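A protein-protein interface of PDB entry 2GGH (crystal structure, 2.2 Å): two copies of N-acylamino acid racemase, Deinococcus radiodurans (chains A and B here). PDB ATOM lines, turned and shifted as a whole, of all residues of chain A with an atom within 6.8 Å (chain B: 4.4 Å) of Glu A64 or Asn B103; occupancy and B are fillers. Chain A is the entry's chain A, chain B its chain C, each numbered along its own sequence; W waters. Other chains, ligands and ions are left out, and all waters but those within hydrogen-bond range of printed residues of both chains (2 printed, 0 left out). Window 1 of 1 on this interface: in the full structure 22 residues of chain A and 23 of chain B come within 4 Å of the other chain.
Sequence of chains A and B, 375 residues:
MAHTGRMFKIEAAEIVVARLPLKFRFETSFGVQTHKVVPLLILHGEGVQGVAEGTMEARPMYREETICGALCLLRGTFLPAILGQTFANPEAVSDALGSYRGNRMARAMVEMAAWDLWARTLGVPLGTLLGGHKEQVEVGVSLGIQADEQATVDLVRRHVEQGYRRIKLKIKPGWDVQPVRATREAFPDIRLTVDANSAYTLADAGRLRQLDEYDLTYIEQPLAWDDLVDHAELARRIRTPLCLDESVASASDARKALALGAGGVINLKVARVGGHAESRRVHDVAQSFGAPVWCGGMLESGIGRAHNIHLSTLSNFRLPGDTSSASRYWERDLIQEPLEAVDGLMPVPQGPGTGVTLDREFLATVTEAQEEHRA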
ATOM      1  N   MET A  56     -24.976 -29.633  20.221  1.00  0.00           N
ATOM      2  CA  MET A  56     -25.244 -28.579  21.200  1.00  0.00           C
ATOM      3  C   MET A  56     -25.344 -29.192  22.608  1.00  0.00           C
ATOM      4  O   MET A  56     -25.716 -30.372  22.764  1.00  0.00           O
ATOM      5  CB  MET A  56     -26.508 -27.796  20.829  1.00  0.00           C
ATOM      6  CG  MET A  56     -27.838 -28.587  20.953  1.00  0.00           C
ATOM      7  SD  MET A  56     -28.133 -29.909  19.743  1.00  0.00           S
ATOM      8  CE  MET A  56     -28.124 -29.011  18.196  1.00  0.00           C
ATOM      9  N   GLU A  57     -24.980 -28.399  23.618  1.00  0.00           N
ATOM     10  CA  GLU A  57     -24.909 -28.844  25.016  1.00  0.00           C
ATOM     11  C   GLU A  57     -26.164 -28.409  25.755  1.00  0.00           C
ATOM     12  O   GLU A  57     -26.998 -27.742  25.176  1.00  0.00           O
ATOM     13  CB  GLU A  57     -23.665 -28.233  25.675  1.00  0.00           C
ATOM     14  CG  GLU A  57     -22.390 -28.441  24.851  1.00  0.00           C
ATOM     15  CD  GLU A  57     -21.310 -27.389  25.102  1.00  0.00           C
ATOM     16  OE1 GLU A  57     -20.184 -27.791  25.467  1.00  0.00           O
ATOM     17  OE2 GLU A  57     -21.565 -26.174  24.915  1.00  0.00           O
ATOM     18  N   ARG A  59     -26.189 -26.295  28.279  1.00  0.00           N
ATOM     19  CA  ARG A  59     -25.921 -24.866  28.398  1.00  0.00           C
ATOM     20  C   ARG A  59     -24.937 -24.449  27.314  1.00  0.00           C
ATOM     21  O   ARG A  59     -24.177 -25.277  26.801  1.00  0.00           O
ATOM     22  CB  ARG A  59     -25.369 -24.532  29.784  1.00  0.00           C
ATOM     23  CG  ARG A  59     -26.261 -25.024  30.894  1.00  0.00           C
ATOM     24  CD  ARG A  59     -25.758 -24.642  32.265  1.00  0.00           C
ATOM     25  NE  ARG A  59     -26.809 -24.870  33.247  1.00  0.00           N
ATOM     26  CZ  ARG A  59     -27.032 -26.039  33.848  1.00  0.00           C
ATOM     27  NH1 ARG A  59     -26.256 -27.092  33.593  1.00  0.00           N
ATOM     28  NH2 ARG A  59     -28.031 -26.156  34.713  1.00  0.00           N
ATOM     29  N   PRO A  60     -24.956 -23.159  26.952  1.00  0.00           N
ATOM     30  CA  PRO A  60     -24.118 -22.609  25.870  1.00  0.00           C
ATOM     31  C   PRO A  60     -22.648 -22.392  26.259  1.00  0.00           C
ATOM     32  O   PRO A  60     -22.259 -21.280  26.641  1.00  0.00           O
ATOM     33  CB  PRO A  60     -24.797 -21.271  25.542  1.00  0.00           C
ATOM     34  CG  PRO A  60     -25.575 -20.902  26.766  1.00  0.00           C
ATOM     35  CD  PRO A  60     -25.836 -22.147  27.572  1.00  0.00           C
ATOM     36  N   MET A  61     -21.828 -23.432  26.124  1.00  0.00           N
ATOM     37  CA  MET A  61     -20.440 -23.369  26.612  1.00  0.00           C
ATOM     38  C   MET A  61     -19.389 -23.361  25.514  1.00  0.00           C
ATOM     39  O   MET A  61     -18.536 -22.484  25.485  1.00  0.00           O
ATOM     40  CB  MET A  61     -20.180 -24.472  27.637  1.00  0.00           C
ATOM     41  CG  MET A  61     -21.215 -24.451  28.765  1.00  0.00           C
ATOM     42  SD  MET A  61     -20.972 -25.675  30.073  1.00  0.00           S
ATOM     43  CE  MET A  61     -19.995 -24.731  31.257  1.00  0.00           C
ATOM     44  N   TYR A  62     -19.455 -24.346  24.623  1.00  0.00           N
ATOM     45  CA  TYR A  62     -18.585 -24.410  23.457  1.00  0.00           C
ATOM     46  C   TYR A  62     -19.010 -23.372  22.432  1.00  0.00           C
ATOM     47  O   TYR A  62     -18.176 -22.741  21.776  1.00  0.00           O
ATOM     48  CB  TYR A  62     -18.634 -25.792  22.808  1.00  0.00           C
ATOM     49  CG  TYR A  62     -18.095 -25.775  21.396  1.00  0.00           C
ATOM     50  CD1 TYR A  62     -16.729 -25.656  21.152  1.00  0.00           C
ATOM     51  CD2 TYR A  62     -18.953 -25.834  20.304  1.00  0.00           C
ATOM     52  CE1 TYR A  62     -16.236 -25.626  19.866  1.00  0.00           C
ATOM     53  CE2 TYR A  62     -18.467 -25.801  19.018  1.00  0.00           C
ATOM     54  CZ  TYR A  62     -17.113 -25.694  18.804  1.00  0.00           C
ATOM     55  OH  TYR A  62     -16.649 -25.663  17.515  1.00  0.00           O
ATOM     56  N   ARG A  63     -20.319 -23.218  22.281  1.00  0.00           N
ATOM     57  CA  ARG A  63     -20.860 -22.151  21.446  1.00  0.00           C
ATOM     58  C   ARG A  63     -22.252 -21.797  21.961  1.00  0.00           C
ATOM     59  O   ARG A  63     -22.588 -22.105  23.101  1.00  0.00           O
ATOM     60  CB  ARG A  63     -20.824 -22.498  19.933  1.00  0.00           C
ATOM     61  CG  ARG A  63     -20.233 -21.356  19.039  1.00  0.00           C
ATOM     62  CD  ARG A  63     -20.113 -21.761  17.553  1.00  0.00           C
ATOM     63  NE  ARG A  63     -19.595 -20.712  16.653  1.00  0.00           N
ATOM     64  CZ  ARG A  63     -20.310 -19.689  16.158  1.00  0.00           C
ATOM     65  NH1 ARG A  63     -19.731 -18.799  15.335  1.00  0.00           N
ATOM     66  NH2 ARG A  63     -21.599 -19.538  16.478  1.00  0.00           N
ATOM     67  N   GLU A  64     -23.055 -21.169  21.118  1.00  0.00           N
ATOM     68  CA  GLU A  64     -24.228 -20.434  21.560  1.00  0.00           C
ATOM     69  C   GLU A  64     -25.510 -21.281  21.718  1.00  0.00           C
ATOM     70  O   GLU A  64     -26.483 -20.853  22.364  1.00  0.00           O
ATOM     71  CB  GLU A  64     -24.466 -19.258  20.586  1.00  0.00           C
ATOM     72  CG  GLU A  64     -25.272 -19.581  19.310  1.00  0.00           C
ATOM     73  CD  GLU A  64     -24.447 -20.212  18.142  1.00  0.00           C
ATOM     74  OE1 GLU A  64     -25.001 -20.293  17.025  1.00  0.00           O
ATOM     75  OE2 GLU A  64     -23.278 -20.629  18.313  1.00  0.00           O
ATOM     76  N   GLU A  65     -25.532 -22.465  21.114  1.00  0.00           N
ATOM     77  CA  GLU A  65     -26.773 -23.237  21.039  1.00  0.00           C
ATOM     78  C   GLU A  65     -26.977 -24.116  22.258  1.00  0.00           C
ATOM     79  O   GLU A  65     -26.040 -24.396  22.999  1.00  0.00           O
ATOM     80  CB  GLU A  65     -26.818 -24.066  19.757  1.00  0.00           C
ATOM     81  CG  GLU A  65     -26.883 -23.215  18.507  1.00  0.00           C
ATOM     82  CD  GLU A  65     -26.951 -24.034  17.240  1.00  0.00           C
ATOM     83  OE1 GLU A  65     -27.977 -24.722  17.027  1.00  0.00           O
ATOM     84  OE2 GLU A  65     -25.973 -23.985  16.449  1.00  0.00           O
ATOM     85  N   THR A  66     -28.220 -24.532  22.477  1.00  0.00           N
ATOM     86  CA  THR A  66     -28.525 -25.466  23.555  1.00  0.00           C
ATOM     87  C   THR A  66     -29.479 -26.543  23.067  1.00  0.00           C
ATOM     88  O   THR A  66     -30.145 -26.375  22.043  1.00  0.00           O
ATOM     89  CB  THR A  66     -29.104 -24.757  24.798  1.00  0.00           C
ATOM     90  OG1 THR A  66     -30.412 -24.244  24.501  1.00  0.00           O
ATOM     91  CG2 THR A  66     -28.197 -23.627  25.231  1.00  0.00           C
ATOM     92  N   GLY A 102     -28.664 -18.214  11.962  1.00  0.00           N
ATOM     93  CA  GLY A 102     -27.815 -18.973  12.884  1.00  0.00           C
ATOM     94  C   GLY A 102     -28.354 -20.371  13.145  1.00  0.00           C
ATOM     95  O   GLY A 102     -28.893 -21.018  12.243  1.00  0.00           O
ATOM     96  N   ASN A 103     -28.218 -20.830  14.382  1.00  0.00           N
ATOM     97  CA  ASN A 103     -28.693 -22.163  14.760  1.00  0.00           C
ATOM     98  C   ASN A 103     -28.170 -23.282  13.849  1.00  0.00           C
ATOM     99  O   ASN A 103     -28.916 -24.157  13.419  1.00  0.00           O
ATOM    100  CB  ASN A 103     -30.222 -22.159  14.841  1.00  0.00           C
ATOM    101  CG  ASN A 103     -30.734 -21.184  15.898  1.00  0.00           C
ATOM    102  OD1 ASN A 103     -31.038 -20.017  15.615  1.00  0.00           O
ATOM    103  ND2 ASN A 103     -30.791 -21.648  17.119  1.00  0.00           N
ATOM    104  N   ARG A 104     -26.867 -23.257  13.580  1.00  0.00           N
ATOM    105  CA  ARG A 104     -26.286 -24.164  12.601  1.00  0.00           C
ATOM    106  C   ARG A 104     -26.255 -25.630  13.037  1.00  0.00           C
ATOM    107  O   ARG A 104     -26.450 -26.518  12.209  1.00  0.00           O
ATOM    108  CB  ARG A 104     -24.928 -23.635  12.115  1.00  0.00           C
ATOM    109  CG  ARG A 104     -25.129 -22.477  11.121  1.00  0.00           C
ATOM    110  CD  ARG A 104     -23.854 -21.906  10.579  1.00  0.00           C
ATOM    111  NE  ARG A 104     -24.092 -20.883   9.558  1.00  0.00           N
ATOM    112  CZ  ARG A 104     -23.963 -21.083   8.244  1.00  0.00           C
ATOM    113  NH1 ARG A 104     -23.594 -22.275   7.772  1.00  0.00           N
ATOM    114  NH2 ARG A 104     -24.198 -20.088   7.389  1.00  0.00           N
ATOM    115  N   MET A 105     -26.041 -25.885  14.326  1.00  0.00           N
ATOM    116  CA  MET A 105     -26.079 -27.257  14.859  1.00  0.00           C
ATOM    117  C   MET A 105     -27.502 -27.870  14.837  1.00  0.00           C
ATOM    118  O   MET A 105     -27.671 -29.044  14.506  1.00  0.00           O
ATOM    119  CB  MET A 105     -25.447 -27.333  16.262  1.00  0.00           C
ATOM    120  CG  MET A 105     -24.000 -26.828  16.332  1.00  0.00           C
ATOM    121  SD  MET A 105     -23.355 -26.935  18.016  1.00  0.00           S
ATOM    122  CE  MET A 105     -21.694 -26.306  17.799  1.00  0.00           C
ATOM    123  N   TRP A 225     -13.397 -16.674  20.903  1.00  0.00           N
ATOM    124  CA  TRP A 225     -14.020 -17.764  20.128  1.00  0.00           C
ATOM    125  C   TRP A 225     -14.711 -17.293  18.853  1.00  0.00           C
ATOM    126  O   TRP A 225     -14.801 -18.027  17.867  1.00  0.00           O
ATOM    127  CB  TRP A 225     -15.035 -18.542  20.986  1.00  0.00           C
ATOM    128  CG  TRP A 225     -16.257 -17.717  21.389  1.00  0.00           C
ATOM    129  CD1 TRP A 225     -16.376 -16.919  22.489  1.00  0.00           C
ATOM    130  CD2 TRP A 225     -17.507 -17.619  20.689  1.00  0.00           C
ATOM    131  NE1 TRP A 225     -17.611 -16.327  22.513  1.00  0.00           N
ATOM    132  CE2 TRP A 225     -18.328 -16.741  21.423  1.00  0.00           C
ATOM    133  CE3 TRP A 225     -18.012 -18.191  19.512  1.00  0.00           C
ATOM    134  CZ2 TRP A 225     -19.634 -16.416  21.024  1.00  0.00           C
ATOM    135  CZ3 TRP A 225     -19.309 -17.870  19.117  1.00  0.00           C
ATOM    136  CH2 TRP A 225     -20.105 -16.993  19.873  1.00  0.00           C
ATOM    137  N   GLU B  65     -31.551 -15.810  18.346  1.00  0.00           N
ATOM    138  CA  GLU B  65     -32.187 -16.260  19.587  1.00  0.00           C
ATOM    139  C   GLU B  65     -33.690 -16.522  19.438  1.00  0.00           C
ATOM    140  O   GLU B  65     -34.343 -15.973  18.558  1.00  0.00           O
ATOM    141  CB  GLU B  65     -31.921 -15.276  20.737  1.00  0.00           C
ATOM    142  CG  GLU B  65     -30.464 -15.257  21.232  1.00  0.00           C
ATOM    143  CD  GLU B  65     -30.223 -14.173  22.269  1.00  0.00           C
ATOM    144  OE1 GLU B  65     -30.609 -14.353  23.452  1.00  0.00           O
ATOM    145  OE2 GLU B  65     -29.649 -13.129  21.900  1.00  0.00           O
ATOM    146  N   LEU B  73     -32.637 -21.008  29.195  1.00  0.00           N
ATOM    147  CA  LEU B  73     -31.420 -20.395  29.703  1.00  0.00           C
ATOM    148  C   LEU B  73     -31.671 -19.560  30.980  1.00  0.00           C
ATOM    149  O   LEU B  73     -30.917 -19.654  31.948  1.00  0.00           O
ATOM    150  CB  LEU B  73     -30.760 -19.555  28.598  1.00  0.00           C
ATOM    151  CG  LEU B  73     -29.372 -19.008  28.946  1.00  0.00           C
ATOM    152  CD1 LEU B  73     -28.462 -20.125  29.459  1.00  0.00           C
ATOM    153  CD2 LEU B  73     -28.732 -18.296  27.748  1.00  0.00           C
ATOM    154  N   ARG B 101     -21.732 -18.400  26.202  1.00  0.00           N
ATOM    155  CA  ARG B 101     -21.469 -17.793  24.909  1.00  0.00           C
ATOM    156  C   ARG B 101     -22.741 -17.316  24.215  1.00  0.00           C
ATOM    157  O   ARG B 101     -23.793 -17.968  24.294  1.00  0.00           O
ATOM    158  CB  ARG B 101     -20.679 -18.765  24.029  1.00  0.00           C
ATOM    159  CG  ARG B 101     -19.311 -19.081  24.647  1.00  0.00           C
ATOM    160  CD  ARG B 101     -18.373 -19.809  23.728  1.00  0.00           C
ATOM    161  NE  ARG B 101     -17.028 -19.808  24.305  1.00  0.00           N
ATOM    162  CZ  ARG B 101     -16.012 -20.552  23.875  1.00  0.00           C
ATOM    163  NH1 ARG B 101     -16.167 -21.387  22.854  1.00  0.00           N
ATOM    164  NH2 ARG B 101     -14.834 -20.460  24.478  1.00  0.00           N
ATOM    165  N   GLY B 102     -22.634 -16.168  23.560  1.00  0.00           N
ATOM    166  CA  GLY B 102     -23.729 -15.591  22.794  1.00  0.00           C
ATOM    167  C   GLY B 102     -24.930 -15.323  23.685  1.00  0.00           C
ATOM    168  O   GLY B 102     -24.788 -14.944  24.840  1.00  0.00           O
ATOM    169  N   ASN B 103     -26.120 -15.527  23.143  1.00  0.00           N
ATOM    170  CA  ASN B 103     -27.334 -15.308  23.910  1.00  0.00           C
ATOM    171  C   ASN B 103     -27.342 -13.933  24.588  1.00  0.00           C
ATOM    172  O   ASN B 103     -27.644 -13.829  25.748  1.00  0.00           O
ATOM    173  CB  ASN B 103     -27.490 -16.422  24.949  1.00  0.00           C
ATOM    174  CG  ASN B 103     -27.689 -17.795  24.311  1.00  0.00           C
ATOM    175  OD1 ASN B 103     -28.808 -18.151  23.947  1.00  0.00           O
ATOM    176  ND2 ASN B 103     -26.603 -18.583  24.196  1.00  0.00           N
ATOM    177  N   ARG B 104     -27.032 -12.878  23.846  1.00  0.00           N
ATOM    178  CA  ARG B 104     -27.032 -11.531  24.408  1.00  0.00           C
ATOM    179  C   ARG B 104     -28.417 -11.049  24.881  1.00  0.00           C
ATOM    180  O   ARG B 104     -28.538 -10.464  25.957  1.00  0.00           O
ATOM    181  CB  ARG B 104     -26.444 -10.540  23.396  1.00  0.00           C
ATOM    182  CG  ARG B 104     -25.018 -10.852  22.986  1.00  0.00           C
ATOM    183  CD  ARG B 104     -24.053  -9.923  23.654  1.00  0.00           C
ATOM    184  NE  ARG B 104     -22.667 -10.314  23.448  1.00  0.00           N
ATOM    185  CZ  ARG B 104     -21.635  -9.656  23.965  1.00  0.00           C
ATOM    186  NH1 ARG B 104     -21.847  -8.579  24.715  1.00  0.00           N
ATOM    187  NH2 ARG B 104     -20.395 -10.077  23.747  1.00  0.00           N
ATOM    188  N   MET B 105     -29.449 -11.268  24.072  1.00  0.00           N
ATOM    189  CA  MET B 105     -30.808 -10.842  24.434  1.00  0.00           C
ATOM    190  C   MET B 105     -31.329 -11.464  25.722  1.00  0.00           C
ATOM    191  O   MET B 105     -31.930 -10.765  26.564  1.00  0.00           O
ATOM    192  CB  MET B 105     -31.779 -11.101  23.292  1.00  0.00           C
ATOM    193  CG  MET B 105     -31.464 -10.250  22.074  1.00  0.00           C
ATOM    194  SD  MET B 105     -32.638 -10.523  20.731  1.00  0.00           S
ATOM    195  CE  MET B 105     -31.971  -9.453  19.479  1.00  0.00           C
ATOM    196  N   ALA B 106     -31.113 -12.771  25.872  1.00  0.00           N
ATOM    197  CA  ALA B 106     -31.410 -13.464  27.124  1.00  0.00           C
ATOM    198  C   ALA B 106     -30.670 -12.811  28.310  1.00  0.00           C
ATOM    199  O   ALA B 106     -31.269 -12.550  29.347  1.00  0.00           O
ATOM    200  CB  ALA B 106     -31.054 -14.967  27.010  1.00  0.00           C
ATOM    201  N   ARG B 107     -29.372 -12.556  28.152  1.00  0.00           N
ATOM    202  CA  ARG B 107     -28.578 -11.899  29.197  1.00  0.00           C
ATOM    203  C   ARG B 107     -29.119 -10.512  29.494  1.00  0.00           C
ATOM    204  O   ARG B 107     -29.131 -10.071  30.643  1.00  0.00           O
ATOM    205  CB  ARG B 107     -27.119 -11.738  28.751  1.00  0.00           C
ATOM    206  CG  ARG B 107     -26.308 -13.002  28.767  1.00  0.00           C
ATOM    207  CD  ARG B 107     -24.934 -12.731  28.213  1.00  0.00           C
ATOM    208  NE  ARG B 107     -23.972 -13.726  28.672  1.00  0.00           N
ATOM    209  CZ  ARG B 107     -23.205 -13.581  29.749  1.00  0.00           C
ATOM    210  NH1 ARG B 107     -23.289 -12.480  30.497  1.00  0.00           N
ATOM    211  NH2 ARG B 107     -22.357 -14.544  30.082  1.00  0.00           N
HETATM  212  O   HOH W   1     -31.204 -22.481  26.482  1.00  0.00           O
HETATM  213  O   HOH W   2     -29.092 -20.815  23.235  1.00  0.00           O
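Water W2 lies within hydrogen-bond range of O of Glu A64 (2.8 Å) and OD1 of Asn B103 (2.8 Å). Water W1 lies within hydrogen-bond range of the side-chain hydroxyl (OG1) of Thr A66 and the backbone NH (N) of Leu B73.
Among the printed residues, merely in contact across the chains: Pro A60 with Leu B73, Pro A60 with Asn B103, Arg A63 with Arg B101, Glu A64 with Arg B101, Trp A225 with Arg B101 and Trp A225 with Gly B102.
Of the 9 printed residues of chain B, 4 touch a printed residue of chain A. Printed residues of chain B that touch a printed residue of chain A: Leu B73, Arg B101, Gly B102 and Asn B103. Hydrophobic or aromatic side chains of chain B within 4 Å of the printed part of chain A: Leu B73. Among the printed residues, no Asp or Glu carboxylate lies within 4 Å of a Lys or Arg side-chain nitrogen of the other chain.
The side-chain amide nitrogen (ND2) of Asn B103 lies within hydrogen-bond range of the backbone carbonyl oxygen (O) of Arg B101, at 2.9 Å. OE2 of Glu A64 is in salt-bridge range of NH2 of Arg A63 (2.7 Å). The side-chain carboxylate (OE2) of Glu A57 lies within hydrogen-bond range of the backbone NH (N) of Tyr A62 (2.8 Å). The side-chain carboxylate of Glu A57 lies within hydrogen-bond range of the backbone NH of Met A61 (3.0 Å).
Of the printed residues of chain B, Pro A60 touches Leu B73 (3.8 Å), Arg B101 (3.0 Å) and Asn B103 (3.5 Å). Of the printed residues of chain B, Arg A63 touches Arg B101 (3.96 Å). Glu A64 touches just these residues of chain B: Arg B101 and Asn B103. Asn B103 touches just these residues of chain A: Pro A60 and Glu A64. The nearest residue of chain B that does not touch Glu A64 is Gly B102 (4.3 Å). The nearest residue of chain A that does not touch Asn B103 is Glu A65 (5.1 Å).
5 positions are printed for both chains. Of the 10 pairs that touch across the chains among the printed residues, none has its exchanged pair printed and touching as well.
O of Pro A60 is in hydrogen-bond range of N of Arg B101 (3.0 Å). The side-chain amide nitrogen (ND2) of Asn B103 sits at hydrogen-bond distance from the backbone carbonyl oxygen (O) of Glu A64. The backbone carbonyl oxygen (O) of Tyr A62 lies within hydrogen-bond range of the guanidinium group (NH1) of Arg B101, 2.7 Å away. The guanidinium group of Arg B101 sits close to the backbone carbonyl oxygen of Met A61, at 3.3 Å.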
